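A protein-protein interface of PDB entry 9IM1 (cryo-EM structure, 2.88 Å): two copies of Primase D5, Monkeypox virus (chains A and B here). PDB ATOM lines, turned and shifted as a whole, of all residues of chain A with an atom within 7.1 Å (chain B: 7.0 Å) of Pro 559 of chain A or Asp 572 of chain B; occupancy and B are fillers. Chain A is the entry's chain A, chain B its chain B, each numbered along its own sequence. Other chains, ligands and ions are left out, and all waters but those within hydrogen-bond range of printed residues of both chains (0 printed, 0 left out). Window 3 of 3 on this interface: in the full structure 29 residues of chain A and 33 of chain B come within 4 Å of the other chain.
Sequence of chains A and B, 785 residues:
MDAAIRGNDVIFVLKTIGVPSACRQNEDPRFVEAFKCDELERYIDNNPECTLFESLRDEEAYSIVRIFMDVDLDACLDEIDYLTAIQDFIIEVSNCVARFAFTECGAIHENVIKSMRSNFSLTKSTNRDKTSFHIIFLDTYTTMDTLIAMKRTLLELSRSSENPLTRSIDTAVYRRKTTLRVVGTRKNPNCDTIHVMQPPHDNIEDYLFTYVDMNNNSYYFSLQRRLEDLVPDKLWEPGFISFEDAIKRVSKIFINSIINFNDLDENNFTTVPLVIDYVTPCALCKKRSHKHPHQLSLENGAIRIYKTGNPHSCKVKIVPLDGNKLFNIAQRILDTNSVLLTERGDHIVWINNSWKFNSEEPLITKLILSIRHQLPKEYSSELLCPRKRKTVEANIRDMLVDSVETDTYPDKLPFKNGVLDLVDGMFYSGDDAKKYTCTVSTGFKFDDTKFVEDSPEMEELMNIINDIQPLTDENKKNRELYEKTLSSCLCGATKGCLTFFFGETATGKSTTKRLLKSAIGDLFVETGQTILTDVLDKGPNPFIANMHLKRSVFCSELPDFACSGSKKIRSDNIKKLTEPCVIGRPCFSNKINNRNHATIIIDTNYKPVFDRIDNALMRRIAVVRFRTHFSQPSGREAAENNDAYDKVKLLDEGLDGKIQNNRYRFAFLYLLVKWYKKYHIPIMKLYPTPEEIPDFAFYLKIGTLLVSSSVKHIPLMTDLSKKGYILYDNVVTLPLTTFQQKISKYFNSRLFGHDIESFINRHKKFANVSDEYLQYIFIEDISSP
NZ of Lys 576 of chain B is in hydrogen-bond range of O of Glu 557 of chain A (3.2 Å). The guanidinium group of Arg 612 of chain B lies close to the side-chain carboxylate of Asp 560 of chain A.
OD1 of Asp 560 of chain A is in hydrogen-bond range of N of Ala 562 of chain A, 3.3 Å away. The backbone carbonyl oxygen (O) of Asp 560 of chain A is in hydrogen-bond range of the side-chain sulfur (SG) of Cys 563 of chain A, 3.7 Å away. The side-chain hydroxyl (OG) of Ser 566 of chain A sits at hydrogen-bond distance from the backbone carbonyl oxygen (O) of Asp 560 of chain A, at 2.8 Å. The side-chain hydroxyl (OG1) of Thr 604 of chain A sits at hydrogen-bond distance from the backbone carbonyl oxygen (O) of Tyr 606 of chain A (3.2 Å). O of Arg 612 of chain B sits at hydrogen-bond distance from OG of Ser 571 of chain B (3.4 Å). The side-chain carboxylate of Asp 572 of chain B lies within salt-bridge range of the side-chain amino group of Lys 576 of chain B, 3.5 Å away.
Glu 557 of chain A touches Lys 575 of chain B (CG to CB, 3.7 Å). Asp 572 of chain B touches Pro 559 of chain A. Tyr 606 of chain A touches Arg 612 of chain B.
Pro 559 of chain A touches one residue of chain B. Of the printed residues of chain A, Arg 612 of chain B touches Asp 560 and Tyr 606. Printed residues of chain B within 4 Å of Asp 560 of chain A: Arg 612 (2.3 Å). Of the printed residues of chain A, Lys 575 of chain B touches Glu 557 (3.7 Å). The nearest residue of chain A that does not touch Asp 572 of chain B is Glu 557 of chain A (4.1 Å). The nearest printed residue of chain A that does not touch Lys 576 of chain B is Ser 556 of chain A (4.03 Å).
Of the 16 printed residues of chain A, 4 touch a printed residue of chain B. Hydrophobic or aromatic side chains of chain A within 4 Å of the printed part of chain B: Pro 559 and Tyr 606. Of the 13 printed residues of chain B, 4 touch a printed residue of chain A.
No position is printed for both chains. Of the 5 pairs that touch across the chains among the printed residues, none has its exchanged pair printed and touching as well.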
ATOM      1  N   GLN A 529     -19.661   9.437  24.895  1.00  0.00           N
ATOM      2  CA  GLN A 529     -18.749  10.479  24.442  1.00  0.00           C
ATOM      3  C   GLN A 529     -17.281  10.165  24.697  1.00  0.00           C
ATOM      4  O   GLN A 529     -16.423  10.952  24.283  1.00  0.00           O
ATOM      5  CB  GLN A 529     -19.180  11.826  25.057  1.00  0.00           C
ATOM      6  CG  GLN A 529     -19.305  11.970  26.602  1.00  0.00           C
ATOM      7  CD  GLN A 529     -18.073  11.672  27.456  1.00  0.00           C
ATOM      8  OE1 GLN A 529     -16.966  11.488  26.967  1.00  0.00           O
ATOM      9  NE2 GLN A 529     -18.281  11.643  28.767  1.00  0.00           N
ATOM     10  N   THR A 533     -13.222  11.828  23.844  1.00  0.00           N
ATOM     11  CA  THR A 533     -12.585  12.476  24.982  1.00  0.00           C
ATOM     12  C   THR A 533     -11.414  11.696  25.558  1.00  0.00           C
ATOM     13  O   THR A 533     -10.392  12.295  25.898  1.00  0.00           O
ATOM     14  CB  THR A 533     -13.626  12.718  26.083  1.00  0.00           C
ATOM     15  OG1 THR A 533     -14.770  13.372  25.521  1.00  0.00           O
ATOM     16  CG2 THR A 533     -13.049  13.590  27.175  1.00  0.00           C
ATOM     17  N   SER A 556     -24.582  12.026  21.928  1.00  0.00           N
ATOM     18  CA  SER A 556     -25.616  12.902  22.448  1.00  0.00           C
ATOM     19  C   SER A 556     -25.098  13.722  23.619  1.00  0.00           C
ATOM     20  O   SER A 556     -24.228  13.291  24.382  1.00  0.00           O
ATOM     21  CB  SER A 556     -26.844  12.094  22.884  1.00  0.00           C
ATOM     22  OG  SER A 556     -26.525  11.243  23.977  1.00  0.00           O
ATOM     23  N   GLU A 557     -25.664  14.923  23.747  1.00  0.00           N
ATOM     24  CA  GLU A 557     -25.509  15.773  24.923  1.00  0.00           C
ATOM     25  C   GLU A 557     -24.041  16.098  25.201  1.00  0.00           C
ATOM     26  O   GLU A 557     -23.467  15.700  26.215  1.00  0.00           O
ATOM     27  CB  GLU A 557     -26.182  15.126  26.138  1.00  0.00           C
ATOM     28  CG  GLU A 557     -27.714  14.967  26.060  1.00  0.00           C
ATOM     29  CD  GLU A 557     -28.445  15.970  25.160  1.00  0.00           C
ATOM     30  OE1 GLU A 557     -28.032  17.147  25.054  1.00  0.00           O
ATOM     31  OE2 GLU A 557     -29.452  15.567  24.542  1.00  0.00           O
ATOM     32  N   LEU A 558     -23.436  16.817  24.264  1.00  0.00           N
ATOM     33  CA  LEU A 558     -22.129  17.398  24.520  1.00  0.00           C
ATOM     34  C   LEU A 558     -22.252  18.486  25.586  1.00  0.00           C
ATOM     35  O   LEU A 558     -23.160  19.321  25.520  1.00  0.00           O
ATOM     36  CB  LEU A 558     -21.538  17.987  23.241  1.00  0.00           C
ATOM     37  CG  LEU A 558     -20.739  17.038  22.349  1.00  0.00           C
ATOM     38  CD1 LEU A 558     -20.029  17.805  21.243  1.00  0.00           C
ATOM     39  CD2 LEU A 558     -19.746  16.242  23.176  1.00  0.00           C
ATOM     40  N   PRO A 559     -21.366  18.505  26.575  1.00  0.00           N
ATOM     41  CA  PRO A 559     -21.451  19.516  27.630  1.00  0.00           C
ATOM     42  C   PRO A 559     -20.856  20.844  27.180  1.00  0.00           C
ATOM     43  O   PRO A 559     -20.149  20.938  26.177  1.00  0.00           O
ATOM     44  CB  PRO A 559     -20.633  18.896  28.762  1.00  0.00           C
ATOM     45  CG  PRO A 559     -19.581  18.119  28.050  1.00  0.00           C
ATOM     46  CD  PRO A 559     -20.219  17.602  26.774  1.00  0.00           C
ATOM     47  N   ASP A 560     -21.162  21.883  27.953  1.00  0.00           N
ATOM     48  CA  ASP A 560     -20.600  23.201  27.692  1.00  0.00           C
ATOM     49  C   ASP A 560     -19.138  23.221  28.120  1.00  0.00           C
ATOM     50  O   ASP A 560     -18.819  22.935  29.279  1.00  0.00           O
ATOM     51  CB  ASP A 560     -21.393  24.274  28.434  1.00  0.00           C
ATOM     52  CG  ASP A 560     -20.935  25.677  28.093  1.00  0.00           C
ATOM     53  OD1 ASP A 560     -20.216  25.841  27.085  1.00  0.00           O
ATOM     54  OD2 ASP A 560     -21.290  26.614  28.835  1.00  0.00           O
ATOM     55  N   PHE A 561     -18.252  23.560  27.188  1.00  0.00           N
ATOM     56  CA  PHE A 561     -16.822  23.543  27.462  1.00  0.00           C
ATOM     57  C   PHE A 561     -16.331  24.809  28.149  1.00  0.00           C
ATOM     58  O   PHE A 561     -15.177  24.845  28.590  1.00  0.00           O
ATOM     59  CB  PHE A 561     -16.048  23.325  26.161  1.00  0.00           C
ATOM     60  CG  PHE A 561     -16.459  22.087  25.418  1.00  0.00           C
ATOM     61  CD1 PHE A 561     -15.963  20.849  25.784  1.00  0.00           C
ATOM     62  CD2 PHE A 561     -17.346  22.163  24.358  1.00  0.00           C
ATOM     63  CE1 PHE A 561     -16.340  19.708  25.104  1.00  0.00           C
ATOM     64  CE2 PHE A 561     -17.727  21.026  23.674  1.00  0.00           C
ATOM     65  CZ  PHE A 561     -17.224  19.798  24.048  1.00  0.00           C
ATOM     66  N   ALA A 562     -17.169  25.843  28.251  1.00  0.00           N
ATOM     67  CA  ALA A 562     -16.759  27.056  28.951  1.00  0.00           C
ATOM     68  C   ALA A 562     -16.656  26.828  30.453  1.00  0.00           C
ATOM     69  O   ALA A 562     -15.784  27.411  31.107  1.00  0.00           O
ATOM     70  CB  ALA A 562     -17.733  28.193  28.652  1.00  0.00           C
ATOM     71  N   CYS A 563     -17.530  25.996  31.014  1.00  0.00           N
ATOM     72  CA  CYS A 563     -17.496  25.724  32.444  1.00  0.00           C
ATOM     73  C   CYS A 563     -16.223  24.974  32.814  1.00  0.00           C
ATOM     74  O   CYS A 563     -15.709  24.164  32.036  1.00  0.00           O
ATOM     75  CB  CYS A 563     -18.729  24.922  32.863  1.00  0.00           C
ATOM     76  SG  CYS A 563     -18.501  23.129  32.912  1.00  0.00           S
ATOM     77  N   SER A 566     -14.774  20.839  32.222  1.00  0.00           N
ATOM     78  CA  SER A 566     -15.218  20.168  31.009  1.00  0.00           C
ATOM     79  C   SER A 566     -14.019  19.812  30.140  1.00  0.00           C
ATOM     80  O   SER A 566     -13.177  20.664  29.843  1.00  0.00           O
ATOM     81  CB  SER A 566     -16.191  21.055  30.235  1.00  0.00           C
ATOM     82  OG  SER A 566     -17.389  21.252  30.965  1.00  0.00           O
ATOM     83  N   LYS A 567     -13.946  18.550  29.730  1.00  0.00           N
ATOM     84  CA  LYS A 567     -12.844  18.065  28.915  1.00  0.00           C
ATOM     85  C   LYS A 567     -13.127  18.315  27.440  1.00  0.00           C
ATOM     86  O   LYS A 567     -14.242  18.089  26.961  1.00  0.00           O
ATOM     87  CB  LYS A 567     -12.611  16.576  29.166  1.00  0.00           C
ATOM     88  CG  LYS A 567     -12.160  16.263  30.581  1.00  0.00           C
ATOM     89  CD  LYS A 567     -10.822  15.550  30.592  1.00  0.00           C
ATOM     90  CE  LYS A 567     -10.956  14.131  30.073  1.00  0.00           C
ATOM     91  NZ  LYS A 567     -11.762  13.286  30.995  1.00  0.00           N
ATOM     92  N   THR A 604     -26.135  18.314  19.701  1.00  0.00           N
ATOM     93  CA  THR A 604     -25.662  19.134  20.804  1.00  0.00           C
ATOM     94  C   THR A 604     -26.340  20.494  20.768  1.00  0.00           C
ATOM     95  O   THR A 604     -26.904  20.906  19.751  1.00  0.00           O
ATOM     96  CB  THR A 604     -24.142  19.299  20.749  1.00  0.00           C
ATOM     97  OG1 THR A 604     -23.694  20.032  21.896  1.00  0.00           O
ATOM     98  CG2 THR A 604     -23.730  20.028  19.480  1.00  0.00           C
ATOM     99  N   TYR A 606     -24.380  23.124  22.076  1.00  0.00           N
ATOM    100  CA  TYR A 606     -23.234  24.013  22.170  1.00  0.00           C
ATOM    101  C   TYR A 606     -22.214  23.650  21.101  1.00  0.00           C
ATOM    102  O   TYR A 606     -22.050  22.480  20.749  1.00  0.00           O
ATOM    103  CB  TYR A 606     -22.585  23.939  23.560  1.00  0.00           C
ATOM    104  CG  TYR A 606     -23.541  24.242  24.689  1.00  0.00           C
ATOM    105  CD1 TYR A 606     -23.948  25.543  24.949  1.00  0.00           C
ATOM    106  CD2 TYR A 606     -24.035  23.227  25.497  1.00  0.00           C
ATOM    107  CE1 TYR A 606     -24.823  25.824  25.978  1.00  0.00           C
ATOM    108  CE2 TYR A 606     -24.909  23.499  26.530  1.00  0.00           C
ATOM    109  CZ  TYR A 606     -25.299  24.799  26.766  1.00  0.00           C
ATOM    110  OH  TYR A 606     -26.170  25.080  27.792  1.00  0.00           O
ATOM    111  N   LYS A 607     -21.523  24.667  20.592  1.00  0.00           N
ATOM    112  CA  LYS A 607     -20.535  24.446  19.551  1.00  0.00           C
ATOM    113  C   LYS A 607     -19.331  23.685  20.107  1.00  0.00           C
ATOM    114  O   LYS A 607     -18.957  23.860  21.269  1.00  0.00           O
ATOM    115  CB  LYS A 607     -20.081  25.775  18.956  1.00  0.00           C
ATOM    116  CG  LYS A 607     -21.083  26.398  18.000  1.00  0.00           C
ATOM    117  CD  LYS A 607     -21.308  25.511  16.788  1.00  0.00           C
ATOM    118  CE  LYS A 607     -21.874  26.304  15.623  1.00  0.00           C
ATOM    119  NZ  LYS A 607     -23.086  27.075  16.014  1.00  0.00           N
ATOM    120  N   PRO A 608     -18.713  22.828  19.297  1.00  0.00           N
ATOM    121  CA  PRO A 608     -17.564  22.057  19.780  1.00  0.00           C
ATOM    122  C   PRO A 608     -16.349  22.935  20.029  1.00  0.00           C
ATOM    123  O   PRO A 608     -16.162  23.977  19.396  1.00  0.00           O
ATOM    124  CB  PRO A 608     -17.300  21.058  18.644  1.00  0.00           C
ATOM    125  CG  PRO A 608     -18.529  21.092  17.787  1.00  0.00           C
ATOM    126  CD  PRO A 608     -19.080  22.470  17.919  1.00  0.00           C
ATOM    127  N   LEU B 536     -20.729   8.912  33.538  1.00  0.00           N
ATOM    128  CA  LEU B 536     -21.390   7.614  33.559  1.00  0.00           C
ATOM    129  C   LEU B 536     -20.779   6.603  32.599  1.00  0.00           C
ATOM    130  O   LEU B 536     -21.151   5.426  32.648  1.00  0.00           O
ATOM    131  CB  LEU B 536     -22.876   7.778  33.221  1.00  0.00           C
ATOM    132  CG  LEU B 536     -23.569   9.041  33.729  1.00  0.00           C
ATOM    133  CD1 LEU B 536     -24.812   9.334  32.905  1.00  0.00           C
ATOM    134  CD2 LEU B 536     -23.917   8.895  35.190  1.00  0.00           C
ATOM    135  N   ILE B 569     -24.014  19.511  40.423  1.00  0.00           N
ATOM    136  CA  ILE B 569     -24.704  18.530  39.592  1.00  0.00           C
ATOM    137  C   ILE B 569     -24.395  18.803  38.127  1.00  0.00           C
ATOM    138  O   ILE B 569     -24.525  19.937  37.653  1.00  0.00           O
ATOM    139  CB  ILE B 569     -26.217  18.566  39.854  1.00  0.00           C
ATOM    140  CG1 ILE B 569     -26.520  18.131  41.288  1.00  0.00           C
ATOM    141  CG2 ILE B 569     -26.953  17.681  38.864  1.00  0.00           C
ATOM    142  CD1 ILE B 569     -27.961  18.325  41.687  1.00  0.00           C
ATOM    143  N   ARG B 570     -23.977  17.763  37.411  1.00  0.00           N
ATOM    144  CA  ARG B 570     -23.732  17.879  35.980  1.00  0.00           C
ATOM    145  C   ARG B 570     -25.026  18.204  35.250  1.00  0.00           C
ATOM    146  O   ARG B 570     -25.991  17.436  35.307  1.00  0.00           O
ATOM    147  CB  ARG B 570     -23.135  16.579  35.446  1.00  0.00           C
ATOM    148  CG  ARG B 570     -21.779  16.233  36.022  1.00  0.00           C
ATOM    149  CD  ARG B 570     -20.719  17.206  35.554  1.00  0.00           C
ATOM    150  NE  ARG B 570     -20.578  17.183  34.104  1.00  0.00           N
ATOM    151  CZ  ARG B 570     -19.807  16.332  33.441  1.00  0.00           C
ATOM    152  NH1 ARG B 570     -19.089  15.415  34.069  1.00  0.00           N
ATOM    153  NH2 ARG B 570     -19.756  16.402  32.114  1.00  0.00           N
ATOM    154  N   SER B 571     -25.045  19.346  34.560  1.00  0.00           N
ATOM    155  CA  SER B 571     -26.244  19.741  33.830  1.00  0.00           C
ATOM    156  C   SER B 571     -26.529  18.802  32.665  1.00  0.00           C
ATOM    157  O   SER B 571     -27.694  18.583  32.319  1.00  0.00           O
ATOM    158  CB  SER B 571     -26.106  21.178  33.331  1.00  0.00           C
ATOM    159  OG  SER B 571     -27.169  21.515  32.459  1.00  0.00           O
ATOM    160  N   ASP B 572     -25.487  18.244  32.050  1.00  0.00           N
ATOM    161  CA  ASP B 572     -25.666  17.329  30.932  1.00  0.00           C
ATOM    162  C   ASP B 572     -25.982  15.906  31.368  1.00  0.00           C
ATOM    163  O   ASP B 572     -26.428  15.109  30.537  1.00  0.00           O
ATOM    164  CB  ASP B 572     -24.414  17.323  30.053  1.00  0.00           C
ATOM    165  CG  ASP B 572     -23.190  16.829  30.793  1.00  0.00           C
ATOM    166  OD1 ASP B 572     -23.149  16.968  32.032  1.00  0.00           O
ATOM    167  OD2 ASP B 572     -22.269  16.301  30.137  1.00  0.00           O
ATOM    168  N   ASN B 573     -25.764  15.565  32.639  1.00  0.00           N
ATOM    169  CA  ASN B 573     -26.065  14.212  33.093  1.00  0.00           C
ATOM    170  C   ASN B 573     -27.567  13.981  33.181  1.00  0.00           C
ATOM    171  O   ASN B 573     -28.053  12.895  32.843  1.00  0.00           O
ATOM    172  CB  ASN B 573     -25.402  13.943  34.441  1.00  0.00           C
ATOM    173  CG  ASN B 573     -24.082  13.217  34.303  1.00  0.00           C
ATOM    174  OD1 ASN B 573     -23.445  13.261  33.254  1.00  0.00           O
ATOM    175  ND2 ASN B 573     -23.666  12.538  35.365  1.00  0.00           N
ATOM    176  N   ILE B 574     -28.321  14.986  33.631  1.00  0.00           N
ATOM    177  CA  ILE B 574     -29.765  14.818  33.740  1.00  0.00           C
ATOM    178  C   ILE B 574     -30.432  14.808  32.372  1.00  0.00           C
ATOM    179  O   ILE B 574     -31.576  14.354  32.251  1.00  0.00           O
ATOM    180  CB  ILE B 574     -30.348  15.894  34.681  1.00  0.00           C
ATOM    181  CG1 ILE B 574     -30.413  17.289  34.039  1.00  0.00           C
ATOM    182  CG2 ILE B 574     -29.547  15.954  35.974  1.00  0.00           C
ATOM    183  CD1 ILE B 574     -31.634  17.568  33.164  1.00  0.00           C
ATOM    184  N   LYS B 575     -29.751  15.302  31.335  1.00  0.00           N
ATOM    185  CA  LYS B 575     -30.284  15.185  29.984  1.00  0.00           C
ATOM    186  C   LYS B 575     -30.164  13.761  29.460  1.00  0.00           C
ATOM    187  O   LYS B 575     -31.022  13.308  28.695  1.00  0.00           O
ATOM    188  CB  LYS B 575     -29.568  16.156  29.048  1.00  0.00           C
ATOM    189  CG  LYS B 575     -29.869  17.618  29.324  1.00  0.00           C
ATOM    190  CD  LYS B 575     -29.054  18.524  28.419  1.00  0.00           C
ATOM    191  CE  LYS B 575     -29.232  19.983  28.795  1.00  0.00           C
ATOM    192  NZ  LYS B 575     -28.232  20.852  28.122  1.00  0.00           N
ATOM    193  N   LYS B 576     -29.109  13.045  29.856  1.00  0.00           N
ATOM    194  CA  LYS B 576     -28.963  11.654  29.441  1.00  0.00           C
ATOM    195  C   LYS B 576     -29.923  10.742  30.190  1.00  0.00           C
ATOM    196  O   LYS B 576     -30.329   9.702  29.659  1.00  0.00           O
ATOM    197  CB  LYS B 576     -27.523  11.192  29.652  1.00  0.00           C
ATOM    198  CG  LYS B 576     -26.509  11.916  28.791  1.00  0.00           C
ATOM    199  CD  LYS B 576     -25.101  11.429  29.079  1.00  0.00           C
ATOM    200  CE  LYS B 576     -24.077  12.190  28.258  1.00  0.00           C
ATOM    201  NZ  LYS B 576     -24.026  13.626  28.639  1.00  0.00           N
ATOM    202  N   LEU B 577     -30.298  11.110  31.412  1.00  0.00           N
ATOM    203  CA  LEU B 577     -31.222  10.314  32.208  1.00  0.00           C
ATOM    204  C   LEU B 577     -32.660  10.422  31.723  1.00  0.00           C
ATOM    205  O   LEU B 577     -33.532   9.730  32.258  1.00  0.00           O
ATOM    206  CB  LEU B 577     -31.137  10.730  33.678  1.00  0.00           C
ATOM    207  CG  LEU B 577     -29.796  10.459  34.360  1.00  0.00           C
ATOM    208  CD1 LEU B 577     -29.790  11.008  35.776  1.00  0.00           C
ATOM    209  CD2 LEU B 577     -29.486   8.973  34.360  1.00  0.00           C
ATOM    210  N   ASP B 611     -24.327  23.228  37.289  1.00  0.00           N
ATOM    211  CA  ASP B 611     -23.180  23.865  36.649  1.00  0.00           C
ATOM    212  C   ASP B 611     -23.618  24.979  35.707  1.00  0.00           C
ATOM    213  O   ASP B 611     -23.109  26.104  35.779  1.00  0.00           O
ATOM    214  CB  ASP B 611     -22.361  22.824  35.886  1.00  0.00           C
ATOM    215  CG  ASP B 611     -21.654  21.854  36.802  1.00  0.00           C
ATOM    216  OD1 ASP B 611     -21.316  22.247  37.937  1.00  0.00           O
ATOM    217  OD2 ASP B 611     -21.433  20.698  36.385  1.00  0.00           O
ATOM    218  N   ARG B 612     -24.560  24.685  34.816  1.00  0.00           N
ATOM    219  CA  ARG B 612     -25.022  25.628  33.809  1.00  0.00           C
ATOM    220  C   ARG B 612     -26.541  25.614  33.759  1.00  0.00           C
ATOM    221  O   ARG B 612     -27.167  24.563  33.930  1.00  0.00           O
ATOM    222  CB  ARG B 612     -24.442  25.289  32.428  1.00  0.00           C
ATOM    223  CG  ARG B 612     -24.902  26.209  31.310  1.00  0.00           C
ATOM    224  CD  ARG B 612     -24.371  27.619  31.487  1.00  0.00           C
ATOM    225  NE  ARG B 612     -24.828  28.503  30.422  1.00  0.00           N
ATOM    226  CZ  ARG B 612     -24.188  28.692  29.275  1.00  0.00           C
ATOM    227  NH1 ARG B 612     -23.053  28.070  29.008  1.00  0.00           N
ATOM    228  NH2 ARG B 612     -24.704  29.523  28.375  1.00  0.00           N
ATOM    229  N   LEU B 617     -32.524  22.694  30.397  1.00  0.00           N
ATOM    230  CA  LEU B 617     -32.515  22.222  31.776  1.00  0.00           C
ATOM    231  C   LEU B 617     -33.838  22.499  32.481  1.00  0.00           C
ATOM    232  O   LEU B 617     -34.305  21.673  33.271  1.00  0.00           O
ATOM    233  CB  LEU B 617     -31.365  22.875  32.541  1.00  0.00           C
ATOM    234  CG  LEU B 617     -31.148  22.415  33.982  1.00  0.00           C
ATOM    235  CD1 LEU B 617     -30.722  20.963  34.019  1.00  0.00           C
ATOM    236  CD2 LEU B 617     -30.124  23.294  34.675  1.00  0.00           C
